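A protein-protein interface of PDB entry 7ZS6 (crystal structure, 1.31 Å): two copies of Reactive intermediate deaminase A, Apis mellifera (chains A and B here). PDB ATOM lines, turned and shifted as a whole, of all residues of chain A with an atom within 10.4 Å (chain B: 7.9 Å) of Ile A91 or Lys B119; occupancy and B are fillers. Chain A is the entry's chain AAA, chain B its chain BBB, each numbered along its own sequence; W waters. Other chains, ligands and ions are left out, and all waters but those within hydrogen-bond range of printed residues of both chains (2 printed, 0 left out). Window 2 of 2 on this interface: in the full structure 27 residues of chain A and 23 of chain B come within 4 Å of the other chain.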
ATOM      1  N   ALA A  56       8.585 -14.841 -30.365  1.00  0.00           N
ATOM      2  CA  ALA A  56       7.507 -15.793 -30.039  1.00  0.00           C
ATOM      3  C   ALA A  56       7.869 -17.247 -30.297  1.00  0.00           C
ATOM      4  O   ALA A  56       7.492 -18.109 -29.443  1.00  0.00           O
ATOM      5  CB  ALA A  56       6.218 -15.402 -30.719  1.00  0.00           C
ATOM      6  N   ILE A  86      -3.174 -20.104 -23.912  1.00  0.00           N
ATOM      7  CA  ILE A  86      -2.035 -19.408 -24.525  1.00  0.00           C
ATOM      8  C   ILE A  86      -2.323 -17.915 -24.505  1.00  0.00           C
ATOM      9  O   ILE A  86      -3.316 -17.445 -25.102  1.00  0.00           O
ATOM     10  CB  ILE A  86      -1.789 -19.908 -25.942  1.00  0.00           C
ATOM     11  CG1 ILE A  86      -1.512 -21.425 -25.947  1.00  0.00           C
ATOM     12  CG2 ILE A  86      -0.662 -19.131 -26.610  1.00  0.00           C
ATOM     13  CD1 ILE A  86      -1.299 -21.999 -27.343  1.00  0.00           C
ATOM     14  N   PHE A  87      -1.490 -17.167 -23.800  1.00  0.00           N
ATOM     15  CA  PHE A  87      -1.564 -15.708 -23.700  1.00  0.00           C
ATOM     16  C   PHE A  87      -0.506 -15.156 -24.608  1.00  0.00           C
ATOM     17  O   PHE A  87       0.694 -15.470 -24.463  1.00  0.00           O
ATOM     18  CB  PHE A  87      -1.317 -15.253 -22.269  1.00  0.00           C
ATOM     19  CG  PHE A  87      -2.109 -15.952 -21.205  1.00  0.00           C
ATOM     20  CD1 PHE A  87      -3.462 -15.753 -21.050  1.00  0.00           C
ATOM     21  CD2 PHE A  87      -1.496 -16.789 -20.316  1.00  0.00           C
ATOM     22  CE1 PHE A  87      -4.161 -16.367 -20.038  1.00  0.00           C
ATOM     23  CE2 PHE A  87      -2.206 -17.381 -19.266  1.00  0.00           C
ATOM     24  CZ  PHE A  87      -3.548 -17.256 -19.194  1.00  0.00           C
ATOM     25  N   LEU A  88      -0.913 -14.372 -25.580  1.00  0.00           N
ATOM     26  CA  LEU A  88      -0.036 -13.836 -26.609  1.00  0.00           C
ATOM     27  C   LEU A  88       0.090 -12.330 -26.466  1.00  0.00           C
ATOM     28  O   LEU A  88      -0.904 -11.641 -26.174  1.00  0.00           O
ATOM     29  CB  LEU A  88      -0.534 -14.117 -28.018  1.00  0.00           C
ATOM     30  CG  LEU A  88      -0.624 -15.580 -28.385  1.00  0.00           C
ATOM     31  CD1 LEU A  88      -1.271 -15.739 -29.744  1.00  0.00           C
ATOM     32  CD2 LEU A  88       0.718 -16.249 -28.356  1.00  0.00           C
ATOM     33  N   GLN A  89       1.300 -11.831 -26.714  1.00  0.00           N
ATOM     34  CA  GLN A  89       1.414 -10.375 -26.867  1.00  0.00           C
ATOM     35  C   GLN A  89       0.908  -9.916 -28.245  1.00  0.00           C
ATOM     36  O   GLN A  89       0.485  -8.759 -28.347  1.00  0.00           O
ATOM     37  CB  GLN A  89       2.840  -9.905 -26.570  1.00  0.00           C
ATOM     38  CG  GLN A  89       2.970  -8.377 -26.602  1.00  0.00           C
ATOM     39  CD  GLN A  89       2.100  -7.755 -25.550  1.00  0.00           C
ATOM     40  OE1 GLN A  89       2.243  -8.038 -24.391  1.00  0.00           O
ATOM     41  NE2 GLN A  89       1.015  -7.074 -25.910  1.00  0.00           N
ATOM     42  N   ASP A  90       0.947 -10.779 -29.241  1.00  0.00           N
ATOM     43  CA  ASP A  90       0.490 -10.411 -30.601  1.00  0.00           C
ATOM     44  C   ASP A  90      -0.260 -11.603 -31.139  1.00  0.00           C
ATOM     45  O   ASP A  90       0.343 -12.640 -31.444  1.00  0.00           O
ATOM     46  CB  ASP A  90       1.700 -10.061 -31.472  1.00  0.00           C
ATOM     47  CG  ASP A  90       1.375  -9.519 -32.826  1.00  0.00           C
ATOM     48  OD1 ASP A  90       0.235  -9.664 -33.254  1.00  0.00           O
ATOM     49  OD2 ASP A  90       2.340  -9.034 -33.473  1.00  0.00           O
ATOM     50  N   ILE A  91      -1.559 -11.425 -31.404  1.00  0.00           N
ATOM     51  CA  ILE A  91      -2.398 -12.505 -31.976  1.00  0.00           C
ATOM     52  C   ILE A  91      -1.807 -12.996 -33.305  1.00  0.00           C
ATOM     53  O   ILE A  91      -2.073 -14.125 -33.677  1.00  0.00           O
ATOM     54  CB  ILE A  91      -3.864 -11.946 -32.092  1.00  0.00           C
ATOM     55  CG1 ILE A  91      -4.836 -13.122 -32.191  1.00  0.00           C
ATOM     56  CG2 ILE A  91      -4.001 -11.013 -33.295  1.00  0.00           C
ATOM     57  CD1 ILE A  91      -4.991 -13.855 -30.951  1.00  0.00           C
ATOM     58  N   ASN A  92      -1.085 -12.134 -34.025  1.00  0.00           N
ATOM     59  CA  ASN A  92      -0.538 -12.556 -35.327  1.00  0.00           C
ATOM     60  C   ASN A  92       0.555 -13.598 -35.189  1.00  0.00           C
ATOM     61  O   ASN A  92       0.899 -14.227 -36.203  1.00  0.00           O
ATOM     62  CB  ASN A  92      -0.015 -11.379 -36.125  1.00  0.00           C
ATOM     63  CG  ASN A  92      -1.134 -10.482 -36.581  1.00  0.00           C
ATOM     64  OD1 ASN A  92      -2.198 -10.938 -36.979  1.00  0.00           O
ATOM     65  ND2 ASN A  92      -0.885  -9.210 -36.464  1.00  0.00           N
ATOM     66  N   ASP A  93       1.045 -13.873 -33.983  1.00  0.00           N
ATOM     67  CA  ASP A  93       1.995 -14.970 -33.751  1.00  0.00           C
ATOM     68  C   ASP A  93       1.291 -16.309 -33.622  1.00  0.00           C
ATOM     69  O   ASP A  93       1.954 -17.347 -33.486  1.00  0.00           O
ATOM     70  CB  ASP A  93       2.821 -14.689 -32.480  1.00  0.00           C
ATOM     71  CG  ASP A  93       3.751 -13.510 -32.590  1.00  0.00           C
ATOM     72  OD1 ASP A  93       4.310 -13.320 -33.727  1.00  0.00           O
ATOM     73  OD2 ASP A  93       3.976 -12.821 -31.586  1.00  0.00           O
ATOM     74  N   PHE A  94      -0.053 -16.345 -33.609  1.00  0.00           N
ATOM     75  CA  PHE A  94      -0.748 -17.598 -33.294  1.00  0.00           C
ATOM     76  C   PHE A  94      -0.340 -18.758 -34.185  1.00  0.00           C
ATOM     77  O   PHE A  94      -0.061 -19.841 -33.652  1.00  0.00           O
ATOM     78  CB  PHE A  94      -2.250 -17.366 -33.315  1.00  0.00           C
ATOM     79  CG  PHE A  94      -3.135 -18.468 -32.790  1.00  0.00           C
ATOM     80  CD1 PHE A  94      -2.646 -19.506 -32.029  1.00  0.00           C
ATOM     81  CD2 PHE A  94      -4.513 -18.268 -32.820  1.00  0.00           C
ATOM     82  CE1 PHE A  94      -3.488 -20.547 -31.657  1.00  0.00           C
ATOM     83  CE2 PHE A  94      -5.377 -19.231 -32.322  1.00  0.00           C
ATOM     84  CZ  PHE A  94      -4.852 -20.346 -31.716  1.00  0.00           C
ATOM     85  N   THR A  95      -0.266 -18.574 -35.509  1.00  0.00           N
ATOM     86  CA  THR A  95       0.071 -19.715 -36.403  1.00  0.00           C
ATOM     87  C   THR A  95       1.478 -20.258 -36.063  1.00  0.00           C
ATOM     88  O   THR A  95       1.659 -21.459 -36.002  1.00  0.00           O
ATOM     89  CB  THR A  95       0.006 -19.272 -37.865  1.00  0.00           C
ATOM     90  OG1 THR A  95      -1.320 -18.785 -38.070  1.00  0.00           O
ATOM     91  CG2 THR A  95       0.321 -20.420 -38.784  1.00  0.00           C
ATOM     92  N   ASP A  96       2.432 -19.365 -35.847  1.00  0.00           N
ATOM     93  CA  ASP A  96       3.805 -19.790 -35.495  1.00  0.00           C
ATOM     94  C   ASP A  96       3.868 -20.531 -34.147  1.00  0.00           C
ATOM     95  O   ASP A  96       4.519 -21.565 -34.002  1.00  0.00           O
ATOM     96  CB  ASP A  96       4.749 -18.612 -35.474  1.00  0.00           C
ATOM     97  CG  ASP A  96       5.068 -18.043 -36.806  1.00  0.00           C
ATOM     98  OD1 ASP A  96       5.048 -18.857 -37.784  1.00  0.00           O
ATOM     99  OD2 ASP A  96       5.446 -16.826 -36.868  1.00  0.00           O
ATOM    100  N   VAL A  97       3.150 -19.989 -33.171  1.00  0.00           N
ATOM    101  CA  VAL A  97       3.077 -20.593 -31.847  1.00  0.00           C
ATOM    102  C   VAL A  97       2.472 -21.970 -31.962  1.00  0.00           C
ATOM    103  O   VAL A  97       2.961 -22.946 -31.367  1.00  0.00           O
ATOM    104  CB  VAL A  97       2.277 -19.689 -30.928  1.00  0.00           C
ATOM    105  CG1 VAL A  97       1.891 -20.415 -29.643  1.00  0.00           C
ATOM    106  CG2 VAL A  97       3.103 -18.440 -30.633  1.00  0.00           C
ATOM    107  N   ASN A  98       1.412 -22.108 -32.755  1.00  0.00           N
ATOM    108  CA  ASN A  98       0.772 -23.379 -33.008  1.00  0.00           C
ATOM    109  C   ASN A  98       1.748 -24.429 -33.612  1.00  0.00           C
ATOM    110  O   ASN A  98       1.653 -25.618 -33.276  1.00  0.00           O
ATOM    111  CB  ASN A  98      -0.417 -23.027 -33.872  1.00  0.00           C
ATOM    112  CG  ASN A  98      -1.223 -24.257 -33.983  1.00  0.00           C
ATOM    113  OD1 ASN A  98      -1.740 -24.766 -32.978  1.00  0.00           O
ATOM    114  ND2 ASN A  98      -1.304 -24.731 -35.200  1.00  0.00           N
ATOM    115  N   SER A 113      -7.558 -22.467 -25.130  1.00  0.00           N
ATOM    116  CA  SER A 113      -8.022 -21.125 -25.438  1.00  0.00           C
ATOM    117  C   SER A 113      -6.812 -20.248 -25.679  1.00  0.00           C
ATOM    118  O   SER A 113      -5.763 -20.513 -25.119  1.00  0.00           O
ATOM    119  CB  SER A 113      -8.749 -20.556 -24.273  1.00  0.00           C
ATOM    120  OG  SER A 113      -9.934 -21.294 -24.016  1.00  0.00           O
ATOM    121  N   THR A 114      -6.950 -19.285 -26.565  1.00  0.00           N
ATOM    122  CA  THR A 114      -5.868 -18.420 -26.966  1.00  0.00           C
ATOM    123  C   THR A 114      -6.375 -17.006 -27.141  1.00  0.00           C
ATOM    124  O   THR A 114      -7.448 -16.794 -27.718  1.00  0.00           O
ATOM    125  CB  THR A 114      -5.230 -18.876 -28.275  1.00  0.00           C
ATOM    126  OG1 THR A 114      -4.811 -20.245 -28.191  1.00  0.00           O
ATOM    127  CG2 THR A 114      -4.014 -18.028 -28.635  1.00  0.00           C
ATOM    128  N   PHE A 115      -5.644 -16.024 -26.661  1.00  0.00           N
ATOM    129  CA  PHE A 115      -6.000 -14.625 -26.928  1.00  0.00           C
ATOM    130  C   PHE A 115      -4.776 -13.754 -26.724  1.00  0.00           C
ATOM    131  O   PHE A 115      -3.795 -14.164 -26.112  1.00  0.00           O
ATOM    132  CB  PHE A 115      -7.176 -14.163 -26.092  1.00  0.00           C
ATOM    133  CG  PHE A 115      -7.013 -14.322 -24.605  1.00  0.00           C
ATOM    134  CD1 PHE A 115      -6.478 -13.322 -23.813  1.00  0.00           C
ATOM    135  CD2 PHE A 115      -7.471 -15.484 -23.992  1.00  0.00           C
ATOM    136  CE1 PHE A 115      -6.307 -13.504 -22.461  1.00  0.00           C
ATOM    137  CE2 PHE A 115      -7.249 -15.675 -22.627  1.00  0.00           C
ATOM    138  CZ  PHE A 115      -6.705 -14.676 -21.881  1.00  0.00           C
ATOM    139  N   GLN A 116      -4.859 -12.530 -27.247  1.00  0.00           N
ATOM    140  CA  GLN A 116      -3.856 -11.503 -27.041  1.00  0.00           C
ATOM    141  C   GLN A 116      -4.191 -10.696 -25.824  1.00  0.00           C
ATOM    142  O   GLN A 116      -5.311 -10.208 -25.703  1.00  0.00           O
ATOM    143  CB  GLN A 116      -3.773 -10.634 -28.291  1.00  0.00           C
ATOM    144  CG  GLN A 116      -2.805  -9.443 -28.142  1.00  0.00           C
ATOM    145  CD  GLN A 116      -2.819  -8.556 -29.345  1.00  0.00           C
ATOM    146  OE1 GLN A 116      -2.753  -9.038 -30.457  1.00  0.00           O
ATOM    147  NE2 GLN A 116      -2.902  -7.279 -29.085  1.00  0.00           N
ATOM    148  N   VAL A 117      -3.202 -10.540 -24.954  1.00  0.00           N
ATOM    149  CA  VAL A 117      -3.295  -9.747 -23.710  1.00  0.00           C
ATOM    150  C   VAL A 117      -2.808  -8.357 -23.944  1.00  0.00           C
ATOM    151  O   VAL A 117      -2.312  -8.048 -25.029  1.00  0.00           O
ATOM    152  CB  VAL A 117      -2.523 -10.444 -22.592  1.00  0.00           C
ATOM    153  CG1 VAL A 117      -3.041 -11.804 -22.281  1.00  0.00           C
ATOM    154  CG2 VAL A 117      -1.047 -10.447 -22.866  1.00  0.00           C
ATOM    155  N   GLY A 118      -2.940  -7.523 -22.943  1.00  0.00           N
ATOM    156  CA  GLY A 118      -2.328  -6.189 -22.956  1.00  0.00           C
ATOM    157  C   GLY A 118      -0.834  -6.214 -22.826  1.00  0.00           C
ATOM    158  O   GLY A 118      -0.120  -5.588 -23.640  1.00  0.00           O
ATOM    159  N   LYS A 119      -0.346  -6.961 -21.817  1.00  0.00           N
ATOM    160  CA  LYS A 119       1.086  -7.103 -21.570  1.00  0.00           C
ATOM    161  C   LYS A 119       1.283  -8.338 -20.722  1.00  0.00           C
ATOM    162  O   LYS A 119       0.465  -8.664 -19.889  1.00  0.00           O
ATOM    163  CB  LYS A 119       1.733  -5.903 -20.839  1.00  0.00           C
ATOM    164  CG  LYS A 119       2.322  -4.754 -21.615  1.00  0.00           C
ATOM    165  CD  LYS A 119       2.992  -3.732 -20.736  1.00  0.00           C
ATOM    166  CE  LYS A 119       3.169  -2.403 -21.463  1.00  0.00           C
ATOM    167  NZ  LYS A 119       3.555  -1.295 -20.540  1.00  0.00           N
ATOM    168  N   LEU A 120       2.438  -8.962 -20.901  1.00  0.00           N
ATOM    169  CA  LEU A 120       2.888 -10.112 -20.097  1.00  0.00           C
ATOM    170  C   LEU A 120       4.018  -9.668 -19.178  1.00  0.00           C
ATOM    171  O   LEU A 120       4.751  -8.682 -19.437  1.00  0.00           O
ATOM    172  CB  LEU A 120       3.359 -11.261 -21.000  1.00  0.00           C
ATOM    173  CG  LEU A 120       2.253 -11.913 -21.822  1.00  0.00           C
ATOM    174  CD1 LEU A 120       2.854 -12.882 -22.826  1.00  0.00           C
ATOM    175  CD2 LEU A 120       1.234 -12.580 -20.947  1.00  0.00           C
ATOM    176  N   ALA A 124       7.289 -10.390 -22.195  1.00  0.00           N
ATOM    177  CA  ALA A 124       7.320 -11.637 -22.980  1.00  0.00           C
ATOM    178  C   ALA A 124       6.326 -11.591 -24.154  1.00  0.00           C
ATOM    179  O   ALA A 124       5.361 -10.819 -24.144  1.00  0.00           O
ATOM    180  CB  ALA A 124       6.992 -12.797 -22.072  1.00  0.00           C
ATOM    181  N   GLN A 125       6.572 -12.472 -25.091  1.00  0.00           N
ATOM    182  CA  GLN A 125       5.651 -12.621 -26.212  1.00  0.00           C
ATOM    183  C   GLN A 125       4.604 -13.692 -26.004  1.00  0.00           C
ATOM    184  O   GLN A 125       3.608 -13.718 -26.742  1.00  0.00           O
ATOM    185  CB  GLN A 125       6.376 -12.887 -27.523  1.00  0.00           C
ATOM    186  CG  GLN A 125       7.446 -11.878 -27.881  1.00  0.00           C
ATOM    187  CD  GLN A 125       6.848 -10.495 -27.868  1.00  0.00           C
ATOM    188  OE1 GLN A 125       5.929 -10.176 -28.615  1.00  0.00           O
ATOM    189  NE2 GLN A 125       7.344  -9.640 -26.998  1.00  0.00           N
ATOM    190  N   LEU A 126       4.825 -14.606 -25.087  1.00  0.00           N
ATOM    191  CA  LEU A 126       4.034 -15.828 -24.920  1.00  0.00           C
ATOM    192  C   LEU A 126       4.039 -16.195 -23.438  1.00  0.00           C
ATOM    193  O   LEU A 126       5.097 -16.150 -22.798  1.00  0.00           O
ATOM    194  CB  LEU A 126       4.822 -16.885 -25.793  1.00  0.00           C
ATOM    195  CG  LEU A 126       4.431 -18.356 -25.801  1.00  0.00           C
ATOM    196  CD1 LEU A 126       4.811 -19.108 -24.536  1.00  0.00           C
ATOM    197  CD2 LEU A 126       3.030 -18.646 -26.153  1.00  0.00           C
ATOM    198  N   PHE B  87     -14.264 -13.567 -22.640  1.00  0.00           N
ATOM    199  CA  PHE B  87     -13.225 -12.718 -23.188  1.00  0.00           C
ATOM    200  C   PHE B  87     -13.855 -11.756 -24.170  1.00  0.00           C
ATOM    201  O   PHE B  87     -14.351 -12.219 -25.213  1.00  0.00           O
ATOM    202  CB  PHE B  87     -12.113 -13.562 -23.832  1.00  0.00           C
ATOM    203  CG  PHE B  87     -11.562 -14.700 -23.030  1.00  0.00           C
ATOM    204  CD1 PHE B  87     -10.796 -14.473 -21.920  1.00  0.00           C
ATOM    205  CD2 PHE B  87     -11.841 -16.004 -23.374  1.00  0.00           C
ATOM    206  CE1 PHE B  87     -10.316 -15.542 -21.185  1.00  0.00           C
ATOM    207  CE2 PHE B  87     -11.352 -17.078 -22.627  1.00  0.00           C
ATOM    208  CZ  PHE B  87     -10.617 -16.829 -21.520  1.00  0.00           C
ATOM    209  N   LEU B  88     -13.813 -10.468 -23.940  1.00  0.00           N
ATOM    210  CA  LEU B  88     -14.447  -9.489 -24.813  1.00  0.00           C
ATOM    211  C   LEU B  88     -13.405  -8.700 -25.570  1.00  0.00           C
ATOM    212  O   LEU B  88     -12.385  -8.289 -25.029  1.00  0.00           O
ATOM    213  CB  LEU B  88     -15.268  -8.503 -23.984  1.00  0.00           C
ATOM    214  CG  LEU B  88     -16.417  -9.107 -23.206  1.00  0.00           C
ATOM    215  CD1 LEU B  88     -17.074  -8.096 -22.320  1.00  0.00           C
ATOM    216  CD2 LEU B  88     -17.446  -9.665 -24.172  1.00  0.00           C
ATOM    217  N   GLN B  89     -13.683  -8.344 -26.813  1.00  0.00           N
ATOM    218  CA  GLN B  89     -12.907  -7.337 -27.506  1.00  0.00           C
ATOM    219  C   GLN B  89     -13.190  -5.935 -26.931  1.00  0.00           C
ATOM    220  O   GLN B  89     -12.279  -5.076 -27.002  1.00  0.00           O
ATOM    221  CB  GLN B  89     -13.145  -7.380 -29.002  1.00  0.00           C
ATOM    222  CG  GLN B  89     -12.220  -6.491 -29.815  1.00  0.00           C
ATOM    223  CD  GLN B  89     -10.763  -6.804 -29.571  1.00  0.00           C
ATOM    224  OE1 GLN B  89     -10.311  -7.905 -29.820  1.00  0.00           O
ATOM    225  NE2 GLN B  89      -9.990  -5.836 -29.087  1.00  0.00           N
ATOM    226  N   GLN B 116     -11.929  -7.465 -20.864  1.00  0.00           N
ATOM    227  CA  GLN B 116     -11.573  -7.097 -22.228  1.00  0.00           C
ATOM    228  C   GLN B 116     -10.150  -7.475 -22.495  1.00  0.00           C
ATOM    229  O   GLN B 116      -9.261  -7.105 -21.705  1.00  0.00           O
ATOM    230  CB  GLN B 116     -11.789  -5.597 -22.435  1.00  0.00           C
ATOM    231  CG  GLN B 116     -11.306  -5.080 -23.773  1.00  0.00           C
ATOM    232  CD  GLN B 116     -11.507  -3.600 -23.960  1.00  0.00           C
ATOM    233  OE1 GLN B 116     -12.538  -3.057 -23.629  1.00  0.00           O
ATOM    234  NE2 GLN B 116     -10.477  -2.977 -24.486  1.00  0.00           N
ATOM    235  N   VAL B 117      -9.909  -8.210 -23.575  1.00  0.00           N
ATOM    236  CA  VAL B 117      -8.590  -8.621 -23.994  1.00  0.00           C
ATOM    237  C   VAL B 117      -8.019  -7.655 -24.996  1.00  0.00           C
ATOM    238  O   VAL B 117      -8.695  -6.680 -25.366  1.00  0.00           O
ATOM    239  CB  VAL B 117      -8.642 -10.010 -24.631  1.00  0.00           C
ATOM    240  CG1 VAL B 117      -9.147 -10.998 -23.576  1.00  0.00           C
ATOM    241  CG2 VAL B 117      -9.458 -10.020 -25.929  1.00  0.00           C
ATOM    242  N   GLY B 118      -6.772  -7.865 -25.369  1.00  0.00           N
ATOM    243  CA  GLY B 118      -6.184  -7.119 -26.482  1.00  0.00           C
ATOM    244  C   GLY B 118      -6.781  -7.421 -27.817  1.00  0.00           C
ATOM    245  O   GLY B 118      -7.172  -6.517 -28.558  1.00  0.00           O
ATOM    246  N   LYS B 119      -6.751  -8.684 -28.233  1.00  0.00           N
ATOM    247  CA  LYS B 119      -7.381  -9.147 -29.476  1.00  0.00           C
ATOM    248  C   LYS B 119      -7.855 -10.573 -29.248  1.00  0.00           C
ATOM    249  O   LYS B 119      -7.284 -11.302 -28.412  1.00  0.00           O
ATOM    250  CB  LYS B 119      -6.438  -9.057 -30.686  1.00  0.00           C
ATOM    251  CG  LYS B 119      -5.989  -7.647 -31.072  1.00  0.00           C
ATOM    252  CD  LYS B 119      -5.261  -7.480 -32.379  1.00  0.00           C
ATOM    253  CE  LYS B 119      -4.725  -6.067 -32.591  1.00  0.00           C
ATOM    254  NZ  LYS B 119      -3.570  -5.742 -31.687  1.00  0.00           N
ATOM    255  N   LEU B 120      -8.798 -11.031 -30.062  1.00  0.00           N
ATOM    256  CA  LEU B 120      -9.200 -12.423 -30.157  1.00  0.00           C
ATOM    257  C   LEU B 120      -8.807 -12.991 -31.486  1.00  0.00           C
ATOM    258  O   LEU B 120      -8.674 -12.248 -32.479  1.00  0.00           O
ATOM    259  CB  LEU B 120     -10.701 -12.558 -29.944  1.00  0.00           C
ATOM    260  CG  LEU B 120     -11.216 -12.177 -28.560  1.00  0.00           C
ATOM    261  CD1 LEU B 120     -12.699 -12.043 -28.524  1.00  0.00           C
ATOM    262  CD2 LEU B 120     -10.693 -13.147 -27.522  1.00  0.00           C
ATOM    263  N   PRO B 121      -8.744 -14.311 -31.596  1.00  0.00           N
ATOM    264  CA  PRO B 121      -8.608 -14.910 -32.903  1.00  0.00           C
ATOM    265  C   PRO B 121      -9.770 -14.520 -33.804  1.00  0.00           C
ATOM    266  O   PRO B 121     -10.882 -14.251 -33.358  1.00  0.00           O
ATOM    267  CB  PRO B 121      -8.695 -16.425 -32.589  1.00  0.00           C
ATOM    268  CG  PRO B 121      -8.279 -16.546 -31.194  1.00  0.00           C
ATOM    269  CD  PRO B 121      -8.935 -15.330 -30.560  1.00  0.00           C
ATOM    270  N   MET B 122      -9.489 -14.502 -35.101  1.00  0.00           N
ATOM    271  CA  MET B 122     -10.490 -14.239 -36.142  1.00  0.00           C
ATOM    272  C   MET B 122     -11.116 -12.863 -36.017  1.00  0.00           C
ATOM    273  O   MET B 122     -12.204 -12.605 -36.547  1.00  0.00           O
ATOM    274  CB  MET B 122     -11.645 -15.254 -36.152  1.00  0.00           C
ATOM    275  CG  MET B 122     -11.304 -16.640 -36.348  1.00  0.00           C
ATOM    276  SD  MET B 122     -12.932 -17.460 -36.595  1.00  0.00           S
ATOM    277  CE  MET B 122     -13.139 -17.649 -38.330  1.00  0.00           C
ATOM    278  N   ALA B 123     -10.446 -11.939 -35.359  1.00  0.00           N
ATOM    279  CA  ALA B 123     -10.997 -10.608 -35.112  1.00  0.00           C
ATOM    280  C   ALA B 123     -12.390 -10.719 -34.502  1.00  0.00           C
ATOM    281  O   ALA B 123     -13.251  -9.877 -34.701  1.00  0.00           O
ATOM    282  CB  ALA B 123     -10.958  -9.735 -36.317  1.00  0.00           C
ATOM    283  N   ALA B 124     -12.597 -11.701 -33.662  1.00  0.00           N
ATOM    284  CA  ALA B 124     -13.912 -11.883 -33.020  1.00  0.00           C
ATOM    285  C   ALA B 124     -14.227 -10.846 -31.964  1.00  0.00           C
ATOM    286  O   ALA B 124     -13.297 -10.215 -31.403  1.00  0.00           O
ATOM    287  CB  ALA B 124     -13.917 -13.258 -32.393  1.00  0.00           C
ATOM    288  N   GLU B 127     -15.105 -14.474 -27.007  1.00  0.00           N
ATOM    289  CA  GLU B 127     -14.748 -15.876 -26.891  1.00  0.00           C
ATOM    290  C   GLU B 127     -15.238 -16.305 -25.514  1.00  0.00           C
ATOM    291  O   GLU B 127     -15.050 -15.553 -24.564  1.00  0.00           O
ATOM    292  CB  GLU B 127     -13.251 -16.082 -27.071  1.00  0.00           C
ATOM    293  CG  GLU B 127     -12.733 -17.509 -26.975  1.00  0.00           C
ATOM    294  CD  GLU B 127     -11.249 -17.721 -27.195  1.00  0.00           C
ATOM    295  OE1 GLU B 127     -10.620 -16.780 -27.786  1.00  0.00           O
ATOM    296  OE2 GLU B 127     -10.583 -18.689 -26.656  1.00  0.00           O
HETATM  297  O   HOH W   1      -1.974  -7.857 -32.849  1.00  0.00           O
HETATM  298  O   HOH W   2      -8.972 -19.251 -28.646  1.00  0.00           O
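Among the printed residues, pairs that only touch across the chains: Phe A115 with Phe B87 (3.4 Å), Gln A116 with Val B117 (3.5 Å), Thr A114 with Pro B121 (3.5 Å), Ser A113 with Glu B127 (3.5 Å), Phe A115 with Val B117 (3.5 Å), Phe A115 with Lys B119 (3.7 Å), Ile A91 with Pro B121 (3.8 Å), Ile A91 with Lys B119 (3.9 Å), Phe A115 with Leu B120 (3.9 Å) and Ile A91 with Leu B120 (3.9 Å).
Printed residues of chain A that touch a printed residue of chain B: Ile A91, Ser A113, Thr A114, Phe A115 and Gln A116.
Printed residues of chain B that touch a printed residue of chain A: Phe B87, Val B117, Gly B118, Lys B119, Leu B120, Pro B121 and Glu B127.
Hydrophobic or aromatic side chains of chain B that line the printed part of chain A: Phe B87, Val B117, Leu B120 and Pro B121.
Among the printed residues, 13 pairs touch across the chains.
Among the printed residues, no Asp or Glu carboxylate lies within 4 Å of a Lys or Arg side-chain nitrogen of the other chain.
Water W2 bridges OE2 of Glu B127 (2.6 Å) and N of Thr A114 (2.9 Å).
Water W1 lies within hydrogen-bond range of the side-chain amide oxygen of Gln A116 (2.8 Å), the side-chain carboxylate of Asp A90 (2.9 Å) and the side-chain amino group of Lys B119 (2.9 Å).
The backbone carbonyl oxygen of Gln A116 sits at hydrogen-bond distance from the backbone NH of Gly B118 (2.8 Å).
The backbone NH (N) of Gln A116 lies within hydrogen-bond range of the backbone carbonyl oxygen (O) of Lys B119 (3.0 Å).
O of Thr A114 lies close to OE1 of Glu B127 (3.2 Å).
The backbone NH (N) of Ile A86 sits at hydrogen-bond distance from the backbone carbonyl oxygen (O) of Ser A113 (2.9 Å).
The backbone carbonyl oxygen of Ile A86 lies within hydrogen-bond range of the backbone NH of Phe A115 (3.1 Å).
The backbone NH (N) of Ile A91 sits at hydrogen-bond distance from the side-chain amide oxygen (OE1) of Gln A116 (2.8 Å).
The backbone carbonyl oxygen (O) of Glu B127 is in hydrogen-bond range of the backbone NH (N) of Phe B87.
NE2 of Gln B89 sits at hydrogen-bond distance from O of Gly B118 (2.9 Å).
N of Leu B120 lies within hydrogen-bond range of OE1 of Gln B89 (3.5 Å).
Gln A116 touches Val B117, but with the chains exchanged Val A117 does not touch Gln B116 (6.8 Å).
Gln A116 touches Gly B118, but with the chains exchanged Gly A118 does not touch Gln B116 (6.5 Å).
Gln A116 touches Lys B119, but with the chains exchanged Lys A119 does not touch Gln B116 (8.9 Å).
Positions printed for both chains: 87, 88, 89, 116, 117, 118, 119, 120 and 124.
Of the 13 pairs that touch across the chains among the printed residues, none has its exchanged pair printed and touching as well.
Printed residues of chain B within 4 Å of Ile A91: Lys B119 (3.9 Å), Leu B120 (3.9 Å) and Pro B121 (3.8 Å).
Of the printed residues of chain A, Lys B119 touches Ile A91, Phe A115 and Gln A116.
Of chain A, only Phe A115 (3.5 Å) and Gln A116 (3.5 Å) come within 4 Å of Val B117.
Of chain A, only Gln A116 comes within 4 Å of Gly B118.
Of the printed residues of chain A, Pro B121 touches Ile A91 and Thr A114.
Of the printed residues of chain B, Gln A116 touches Val B117 (3.5 Å), Gly B118 (2.8 Å) and Lys B119 (3.0 Å).
Ala A124 touches none of the printed residues of chain B.
Gln B116 touches none of the printed residues of chain A.
The nearest printed residue of chain B that does not touch Ile A91 is Met B122 (5.7 Å).
The nearest printed residue of chain A that does not touch Lys B119 is Val A117 (5.2 Å).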
